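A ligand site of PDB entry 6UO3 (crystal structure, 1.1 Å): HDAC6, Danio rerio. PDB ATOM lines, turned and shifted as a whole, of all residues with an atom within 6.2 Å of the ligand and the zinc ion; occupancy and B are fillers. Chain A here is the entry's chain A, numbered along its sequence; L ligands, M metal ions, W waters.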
ATOM      1  N   ASP A  26      12.394   9.351  -8.227  1.00  0.00           N
ATOM      2  CA  ASP A  26      11.264   8.710  -7.570  1.00  0.00           C
ATOM      3  C   ASP A  26      10.130   8.635  -8.591  1.00  0.00           C
ATOM      4  O   ASP A  26       9.390   9.601  -8.753  1.00  0.00           O
ATOM      5  CB  ASP A  26      10.838   9.473  -6.321  1.00  0.00           C
ATOM      6  CG  ASP A  26       9.613   8.870  -5.650  1.00  0.00           C
ATOM      7  OD1 ASP A  26       9.152   7.796  -6.092  1.00  0.00           O
ATOM      8  OD2 ASP A  26       9.114   9.476  -4.683  1.00  0.00           O
ATOM      9  N   SER A  28       7.413   7.237  -8.429  1.00  0.00           N
ATOM     10  CA  SER A  28       6.092   7.307  -7.826  1.00  0.00           C
ATOM     11  C   SER A  28       5.820   8.646  -7.140  1.00  0.00           C
ATOM     12  O   SER A  28       4.852   8.763  -6.390  1.00  0.00           O
ATOM     13  CB  SER A  28       5.889   6.162  -6.825  1.00  0.00           C
ATOM     14  OG  SER A  28       5.989   4.914  -7.480  1.00  0.00           O
ATOM     15  N   HIS A  29       6.647   9.659  -7.397  1.00  0.00           N
ATOM     16  CA  HIS A  29       6.433  10.945  -6.743  1.00  0.00           C
ATOM     17  C   HIS A  29       5.045  11.456  -7.092  1.00  0.00           C
ATOM     18  O   HIS A  29       4.644  11.412  -8.261  1.00  0.00           O
ATOM     19  CB  HIS A  29       7.472  11.966  -7.194  1.00  0.00           C
ATOM     20  CG  HIS A  29       7.547  13.161  -6.301  1.00  0.00           C
ATOM     21  ND1 HIS A  29       6.586  14.152  -6.291  1.00  0.00           N
ATOM     22  CD2 HIS A  29       8.457  13.515  -5.356  1.00  0.00           C
ATOM     23  CE1 HIS A  29       6.904  15.065  -5.380  1.00  0.00           C
ATOM     24  NE2 HIS A  29       8.036  14.699  -4.803  1.00  0.00           N
ATOM     25  N   PRO A  30       4.274  11.962  -6.121  1.00  0.00           N
ATOM     26  CA  PRO A  30       2.900  12.375  -6.407  1.00  0.00           C
ATOM     27  C   PRO A  30       2.784  13.647  -7.231  1.00  0.00           C
ATOM     28  O   PRO A  30       1.748  13.842  -7.887  1.00  0.00           O
ATOM     29  CB  PRO A  30       2.268  12.551  -5.019  1.00  0.00           C
ATOM     30  CG  PRO A  30       3.440  12.915  -4.147  1.00  0.00           C
ATOM     31  CD  PRO A  30       4.600  12.085  -4.686  1.00  0.00           C
ATOM     32  N   SER A  97      10.989  18.551   1.460  1.00  0.00           N
ATOM     33  CA  SER A  97       9.964  17.997   0.591  1.00  0.00           C
ATOM     34  C   SER A  97       9.928  18.649  -0.803  1.00  0.00           C
ATOM     35  O   SER A  97       8.884  19.123  -1.254  1.00  0.00           O
ATOM     36  CB  SER A  97       8.596  18.034   1.277  1.00  0.00           C
ATOM     37  OG  SER A  97       7.614  17.416   0.478  1.00  0.00           O
ATOM     38  N   VAL A  98      11.069  18.623  -1.484  1.00  0.00           N
ATOM     39  CA  VAL A  98      11.119  19.074  -2.876  1.00  0.00           C
ATOM     40  C   VAL A  98      12.035  18.181  -3.689  1.00  0.00           C
ATOM     41  O   VAL A  98      12.965  17.557  -3.159  1.00  0.00           O
ATOM     42  CB  VAL A  98      11.602  20.534  -3.036  1.00  0.00           C
ATOM     43  CG1 VAL A  98      10.728  21.460  -2.220  1.00  0.00           C
ATOM     44  CG2 VAL A  98      13.047  20.675  -2.630  1.00  0.00           C
ATOM     45  N   PRO A 137       3.323  24.005  -8.047  1.00  0.00           N
ATOM     46  CA  PRO A 137       2.536  24.795  -7.101  1.00  0.00           C
ATOM     47  C   PRO A 137       3.415  25.841  -6.416  1.00  0.00           C
ATOM     48  O   PRO A 137       4.635  25.879  -6.601  1.00  0.00           O
ATOM     49  CB  PRO A 137       2.052  23.735  -6.109  1.00  0.00           C
ATOM     50  CG  PRO A 137       3.155  22.713  -6.105  1.00  0.00           C
ATOM     51  CD  PRO A 137       3.606  22.642  -7.547  1.00  0.00           C
ATOM     52  N   HIS A 139       2.262  27.650  -2.890  1.00  0.00           N
ATOM     53  CA  HIS A 139       1.912  28.277  -1.602  1.00  0.00           C
ATOM     54  C   HIS A 139       2.894  28.003  -0.463  1.00  0.00           C
ATOM     55  O   HIS A 139       2.846  28.717   0.549  1.00  0.00           O
ATOM     56  CB  HIS A 139       0.458  28.031  -1.187  1.00  0.00           C
ATOM     57  CG  HIS A 139       0.116  26.602  -0.863  1.00  0.00           C
ATOM     58  ND1 HIS A 139      -0.896  26.286   0.027  1.00  0.00           N
ATOM     59  CD2 HIS A 139       0.603  25.435  -1.323  1.00  0.00           C
ATOM     60  CE1 HIS A 139      -1.005  24.977   0.102  1.00  0.00           C
ATOM     61  NE2 HIS A 139      -0.109  24.425  -0.701  1.00  0.00           N
ATOM     62  N   HIS A 140       3.760  27.000  -0.589  1.00  0.00           N
ATOM     63  CA  HIS A 140       4.777  26.739   0.432  1.00  0.00           C
ATOM     64  C   HIS A 140       6.080  27.477   0.172  1.00  0.00           C
ATOM     65  O   HIS A 140       6.922  27.550   1.083  1.00  0.00           O
ATOM     66  CB  HIS A 140       5.096  25.245   0.506  1.00  0.00           C
ATOM     67  CG  HIS A 140       3.930  24.400   0.875  1.00  0.00           C
ATOM     68  ND1 HIS A 140       3.243  24.554   2.062  1.00  0.00           N
ATOM     69  CD2 HIS A 140       3.331  23.367   0.228  1.00  0.00           C
ATOM     70  CE1 HIS A 140       2.264  23.671   2.124  1.00  0.00           C
ATOM     71  NE2 HIS A 140       2.312  22.927   1.022  1.00  0.00           N
ATOM     72  N   GLY A 148       7.999  22.067   0.004  1.00  0.00           N
ATOM     73  CA  GLY A 148       6.707  21.458  -0.287  1.00  0.00           C
ATOM     74  C   GLY A 148       6.299  21.439  -1.743  1.00  0.00           C
ATOM     75  O   GLY A 148       5.161  21.802  -2.085  1.00  0.00           O
ATOM     76  N   PHE A 149       7.205  20.991  -2.607  1.00  0.00           N
ATOM     77  CA  PHE A 149       7.003  20.864  -4.048  1.00  0.00           C
ATOM     78  C   PHE A 149       6.985  22.203  -4.775  1.00  0.00           C
ATOM     79  O   PHE A 149       6.714  22.229  -5.984  1.00  0.00           O
ATOM     80  CB  PHE A 149       5.746  20.063  -4.439  1.00  0.00           C
ATOM     81  CG  PHE A 149       5.605  18.717  -3.746  1.00  0.00           C
ATOM     82  CD1 PHE A 149       4.357  18.118  -3.661  1.00  0.00           C
ATOM     83  CD2 PHE A 149       6.702  18.048  -3.231  1.00  0.00           C
ATOM     84  CE1 PHE A 149       4.189  16.888  -3.061  1.00  0.00           C
ATOM     85  CE2 PHE A 149       6.536  16.805  -2.619  1.00  0.00           C
ATOM     86  CZ  PHE A 149       5.277  16.236  -2.535  1.00  0.00           C
ATOM     87  N   CYS A 150       7.305  23.307  -4.093  1.00  0.00           N
ATOM     88  CA  CYS A 150       7.174  24.666  -4.628  1.00  0.00           C
ATOM     89  C   CYS A 150       8.532  25.340  -4.727  1.00  0.00           C
ATOM     90  O   CYS A 150       9.365  25.240  -3.820  1.00  0.00           O
ATOM     91  CB  CYS A 150       6.294  25.524  -3.705  1.00  0.00           C
ATOM     92  SG  CYS A 150       4.649  24.892  -3.365  1.00  0.00           S
ATOM     93  N   ASP A 177      -6.405  24.367  -0.292  1.00  0.00           N
ATOM     94  CA  ASP A 177      -5.558  23.183  -0.301  1.00  0.00           C
ATOM     95  C   ASP A 177      -5.543  22.578   1.104  1.00  0.00           C
ATOM     96  O   ASP A 177      -5.693  23.277   2.107  1.00  0.00           O
ATOM     97  CB  ASP A 177      -4.154  23.620  -0.718  1.00  0.00           C
ATOM     98  CG  ASP A 177      -3.212  22.470  -0.952  1.00  0.00           C
ATOM     99  OD1 ASP A 177      -2.703  21.877   0.032  1.00  0.00           O
ATOM    100  OD2 ASP A 177      -2.948  22.162  -2.142  1.00  0.00           O
ATOM    101  N   VAL A 178      -5.382  21.253   1.170  1.00  0.00           N
ATOM    102  CA  VAL A 178      -5.423  20.576   2.465  1.00  0.00           C
ATOM    103  C   VAL A 178      -4.224  20.909   3.343  1.00  0.00           C
ATOM    104  O   VAL A 178      -4.262  20.652   4.566  1.00  0.00           O
ATOM    105  CB  VAL A 178      -5.581  19.052   2.269  1.00  0.00           C
ATOM    106  CG1 VAL A 178      -4.216  18.391   2.023  1.00  0.00           C
ATOM    107  CG2 VAL A 178      -6.293  18.417   3.461  1.00  0.00           C
ATOM    108  N   HIS A 179      -3.162  21.449   2.776  1.00  0.00           N
ATOM    109  CA  HIS A 179      -1.977  21.835   3.534  1.00  0.00           C
ATOM    110  C   HIS A 179      -1.994  23.326   3.832  1.00  0.00           C
ATOM    111  O   HIS A 179      -2.564  24.129   3.080  1.00  0.00           O
ATOM    112  CB  HIS A 179      -0.715  21.535   2.728  1.00  0.00           C
ATOM    113  CG  HIS A 179      -0.524  20.080   2.424  1.00  0.00           C
ATOM    114  ND1 HIS A 179      -0.993  19.496   1.259  1.00  0.00           N
ATOM    115  CD2 HIS A 179       0.077  19.101   3.128  1.00  0.00           C
ATOM    116  CE1 HIS A 179      -0.677  18.209   1.282  1.00  0.00           C
ATOM    117  NE2 HIS A 179      -0.041  17.944   2.401  1.00  0.00           N
ATOM    118  N   TRP A 208       1.955  17.138   8.059  1.00  0.00           N
ATOM    119  CA  TRP A 208       2.941  18.017   7.466  1.00  0.00           C
ATOM    120  C   TRP A 208       2.291  19.344   7.097  1.00  0.00           C
ATOM    121  O   TRP A 208       1.161  19.361   6.580  1.00  0.00           O
ATOM    122  CB  TRP A 208       3.502  17.323   6.217  1.00  0.00           C
ATOM    123  CG  TRP A 208       4.718  17.983   5.668  1.00  0.00           C
ATOM    124  CD1 TRP A 208       6.014  17.674   5.942  1.00  0.00           C
ATOM    125  CD2 TRP A 208       4.749  19.085   4.759  1.00  0.00           C
ATOM    126  NE1 TRP A 208       6.852  18.522   5.263  1.00  0.00           N
ATOM    127  CE2 TRP A 208       6.091  19.402   4.538  1.00  0.00           C
ATOM    128  CE3 TRP A 208       3.755  19.848   4.124  1.00  0.00           C
ATOM    129  CZ2 TRP A 208       6.484  20.451   3.693  1.00  0.00           C
ATOM    130  CZ3 TRP A 208       4.145  20.880   3.304  1.00  0.00           C
ATOM    131  CH2 TRP A 208       5.495  21.176   3.093  1.00  0.00           C
ATOM    132  N   HIS A 210       3.768  20.321  10.080  1.00  0.00           N
ATOM    133  CA  HIS A 210       4.065  20.165  11.511  1.00  0.00           C
ATOM    134  C   HIS A 210       4.465  21.459  12.204  1.00  0.00           C
ATOM    135  O   HIS A 210       5.331  21.439  13.089  1.00  0.00           O
ATOM    136  CB  HIS A 210       5.192  19.152  11.749  1.00  0.00           C
ATOM    137  CG  HIS A 210       5.083  17.925  10.903  1.00  0.00           C
ATOM    138  ND1 HIS A 210       4.096  16.985  11.093  1.00  0.00           N
ATOM    139  CD2 HIS A 210       5.837  17.476   9.876  1.00  0.00           C
ATOM    140  CE1 HIS A 210       4.256  15.998  10.223  1.00  0.00           C
ATOM    141  NE2 HIS A 210       5.302  16.276   9.465  1.00  0.00           N
ATOM    142  N   GLY A 268      -5.895  24.124  -4.339  1.00  0.00           N
ATOM    143  CA  GLY A 268      -5.515  22.731  -4.278  1.00  0.00           C
ATOM    144  C   GLY A 268      -6.738  21.851  -4.139  1.00  0.00           C
ATOM    145  O   GLY A 268      -7.794  22.300  -3.684  1.00  0.00           O
ATOM    146  N   ASP A 270      -6.348  18.498  -2.858  1.00  0.00           N
ATOM    147  CA  ASP A 270      -5.985  17.381  -2.017  1.00  0.00           C
ATOM    148  C   ASP A 270      -6.927  17.180  -0.837  1.00  0.00           C
ATOM    149  O   ASP A 270      -6.766  16.197  -0.111  1.00  0.00           O
ATOM    150  CB  ASP A 270      -4.506  17.407  -1.594  1.00  0.00           C
ATOM    151  CG  ASP A 270      -3.986  18.809  -1.271  1.00  0.00           C
ATOM    152  OD1 ASP A 270      -4.793  19.749  -1.070  1.00  0.00           O
ATOM    153  OD2 ASP A 270      -2.738  18.934  -1.224  1.00  0.00           O
ATOM    154  N   LYS A 277      -3.076  11.796  -0.079  1.00  0.00           N
ATOM    155  CA  LYS A 277      -2.388  12.485   1.003  1.00  0.00           C
ATOM    156  C   LYS A 277      -3.325  13.191   1.976  1.00  0.00           C
ATOM    157  O   LYS A 277      -3.049  13.235   3.174  1.00  0.00           O
ATOM    158  CB  LYS A 277      -1.427  13.534   0.425  1.00  0.00           C
ATOM    159  CG  LYS A 277      -0.254  12.927  -0.320  1.00  0.00           C
ATOM    160  CD  LYS A 277       0.559  12.041   0.612  1.00  0.00           C
ATOM    161  CE  LYS A 277       1.812  11.527  -0.054  1.00  0.00           C
ATOM    162  NZ  LYS A 277       2.554  10.614   0.850  1.00  0.00           N
ATOM    163  N   GLU A 307      -2.828  24.442  -6.855  1.00  0.00           N
ATOM    164  CA  GLU A 307      -1.795  24.098  -5.891  1.00  0.00           C
ATOM    165  C   GLU A 307      -1.648  22.577  -5.887  1.00  0.00           C
ATOM    166  O   GLU A 307      -1.227  22.004  -6.908  1.00  0.00           O
ATOM    167  CB  GLU A 307      -2.112  24.703  -4.505  1.00  0.00           C
ATOM    168  CG  GLU A 307      -2.184  26.243  -4.492  1.00  0.00           C
ATOM    169  CD  GLU A 307      -0.836  26.950  -4.487  1.00  0.00           C
ATOM    170  OE1 GLU A 307      -0.836  28.208  -4.531  1.00  0.00           O
ATOM    171  OE2 GLU A 307       0.225  26.276  -4.446  1.00  0.00           O
ATOM    172  N   GLY A 308      -2.007  21.899  -4.788  1.00  0.00           N
ATOM    173  CA  GLY A 308      -1.898  20.467  -4.700  1.00  0.00           C
ATOM    174  C   GLY A 308      -3.135  19.732  -5.202  1.00  0.00           C
ATOM    175  O   GLY A 308      -4.019  20.289  -5.852  1.00  0.00           O
ATOM    176  N   GLY A 309      -3.187  18.441  -4.862  1.00  0.00           N
ATOM    177  CA  GLY A 309      -4.205  17.536  -5.376  1.00  0.00           C
ATOM    178  C   GLY A 309      -3.546  16.453  -6.198  1.00  0.00           C
ATOM    179  O   GLY A 309      -2.966  16.739  -7.256  1.00  0.00           O
ATOM    180  N   TYR A 310      -3.611  15.214  -5.724  1.00  0.00           N
ATOM    181  CA  TYR A 310      -2.751  14.142  -6.219  1.00  0.00           C
ATOM    182  C   TYR A 310      -3.488  12.907  -6.720  1.00  0.00           C
ATOM    183  O   TYR A 310      -2.844  12.031  -7.302  1.00  0.00           O
ATOM    184  CB  TYR A 310      -1.697  13.778  -5.152  1.00  0.00           C
ATOM    185  CG  TYR A 310      -0.950  15.010  -4.791  1.00  0.00           C
ATOM    186  CD1 TYR A 310      -0.008  15.537  -5.658  1.00  0.00           C
ATOM    187  CD2 TYR A 310      -1.272  15.738  -3.654  1.00  0.00           C
ATOM    188  CE1 TYR A 310       0.646  16.714  -5.366  1.00  0.00           C
ATOM    189  CE2 TYR A 310      -0.632  16.917  -3.357  1.00  0.00           C
ATOM    190  CZ  TYR A 310       0.323  17.402  -4.212  1.00  0.00           C
ATOM    191  OH  TYR A 310       0.960  18.580  -3.925  1.00  0.00           O
HETATM  192  C1  LIG L   1       6.120  13.406   2.993  1.00  0.00           C
HETATM  193  C2  LIG L   1       6.523  13.512   0.451  1.00  0.00           C
HETATM  194  C3  LIG L   1       7.863  13.164  -1.535  1.00  0.00           C
HETATM  195  C4  LIG L   1       5.985  11.757  -1.169  1.00  0.00           C
HETATM  196  C5  LIG L   1       2.856  16.764  -0.036  1.00  0.00           C
HETATM  197  C6  LIG L   1       1.911  17.602  -0.538  1.00  0.00           C
HETATM  198  C7  LIG L   1       0.988  19.835  -0.995  1.00  0.00           C
HETATM  199  C8  LIG L   1       2.075  18.969  -0.501  1.00  0.00           C
HETATM  200  C9  LIG L   1       3.259  19.420   0.121  1.00  0.00           C
HETATM  201  C10 LIG L   1       4.219  18.553   0.634  1.00  0.00           C
HETATM  202  C11 LIG L   1       4.044  17.194   0.557  1.00  0.00           C
HETATM  203  C12 LIG L   1       4.961  15.035   1.491  1.00  0.00           C
HETATM  204  C13 LIG L   1       6.222  14.307   1.731  1.00  0.00           C
HETATM  205  C14 LIG L   1       5.722  14.189   4.252  1.00  0.00           C
HETATM  206  C15 LIG L   1       7.413  12.657   3.300  1.00  0.00           C
HETATM  207  C16 LIG L   1       7.590  13.851  -0.364  1.00  0.00           C
HETATM  208  C17 LIG L   1       7.061  12.113  -1.958  1.00  0.00           C
HETATM  209  C18 LIG L   1       5.709  12.467   0.010  1.00  0.00           C
HETATM  210  N1  LIG L   1       4.855  16.255   1.000  1.00  0.00           N
HETATM  211  N2  LIG L   1       0.933  21.180  -0.558  1.00  0.00           N
HETATM  212  O1  LIG L   1       0.064  19.443  -1.665  1.00  0.00           O
HETATM  213  O2  LIG L   1       3.886  14.482   1.716  1.00  0.00           O
HETATM  214  O3  LIG L   1      -0.070  21.989  -0.965  1.00  0.00           O
HETATM  215 ZN    ZN M   1      -1.529  20.423  -0.569  1.00  0.00          ZN
HETATM  216  O   HOH W   1      10.894  14.715  -0.389  1.00  0.00           O
HETATM  217  O   HOH W   2       3.018  12.139   2.897  1.00  0.00           O
HETATM  218  O   HOH W   3       1.198  15.449   2.734  1.00  0.00           O
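The zinc ion is bound by OD1 of Asp 177, OD2 of Asp 270, ND1 of His 179, O1 of the ligand and O3 of the ligand. The zinc ion has five donor atoms within binding distance. Slightly farther from the zinc ion lies the side-chain carboxylate (OD2) of Asp 177 (2.7 Å).
Residues that only touch the ligand: Phe 149 (3.3 Å), Trp 208 (3.5 Å), His 29 (3.6 Å), Pro 30 (3.7 Å), Lys 277 (3.8 Å), Gly 308 (3.8 Å) and Gly 148 (3.8 Å). Hydrophobic or aromatic side chains that line the ligand: His 29, Pro 30, His 139, His 140, Phe 149, His 179, Trp 208 and Tyr 310. The nearest printed residue that does not touch the ligand is Asp 26 (4.3 Å).
Of the 24 residues printed, 3 come within 4 Å of the zinc ion.
Water W2 bridges the side-chain amino group (NZ) of Lys 277 (2.6 Å) and an oxygen (O2) of the ligand (2.8 Å). Water W3 lies within hydrogen-bond range of NE2 of His 179 (2.8 Å) and O2 of the ligand (3.0 Å).
NE2 of His 139 lies close to O3 of the ligand (2.5 Å). An oxygen (O1) of the ligand lies close to the side-chain hydroxyl of Tyr 310. N2 of the ligand lies close to NE2 of His 140, at 2.7 Å. N1 of the ligand sits at hydrogen-bond distance from OG of Ser 97, at 3.0 Å.
The side-chain carboxylate (OD1) of Asp 270 is in hydrogen-bond range of the backbone NH (N) of Val 178 (2.8 Å). A ring nitrogen (NE2) of His 139 is in hydrogen-bond range of a ring nitrogen (NE2) of His 140. N of His 139 sits at hydrogen-bond distance from OE2 of Glu 307, at 2.9 Å. The side-chain sulfur (SG) of Cys 150 lies within hydrogen-bond range of the backbone NH (N) of His 139 (3.7 Å). The backbone NH (N) of Phe 149 sits at hydrogen-bond distance from the backbone carbonyl oxygen (O) of Ser 97. O of Ser 97 sits at hydrogen-bond distance from N of Gly 148 (3.3 Å). The backbone NH of His 29 sits at hydrogen-bond distance from the side-chain carboxylate of Asp 26 (3.4 Å). The side-chain sulfur of Cys 150 lies within hydrogen-bond range of the backbone carbonyl oxygen of Gly 148, at 3.4 Å.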
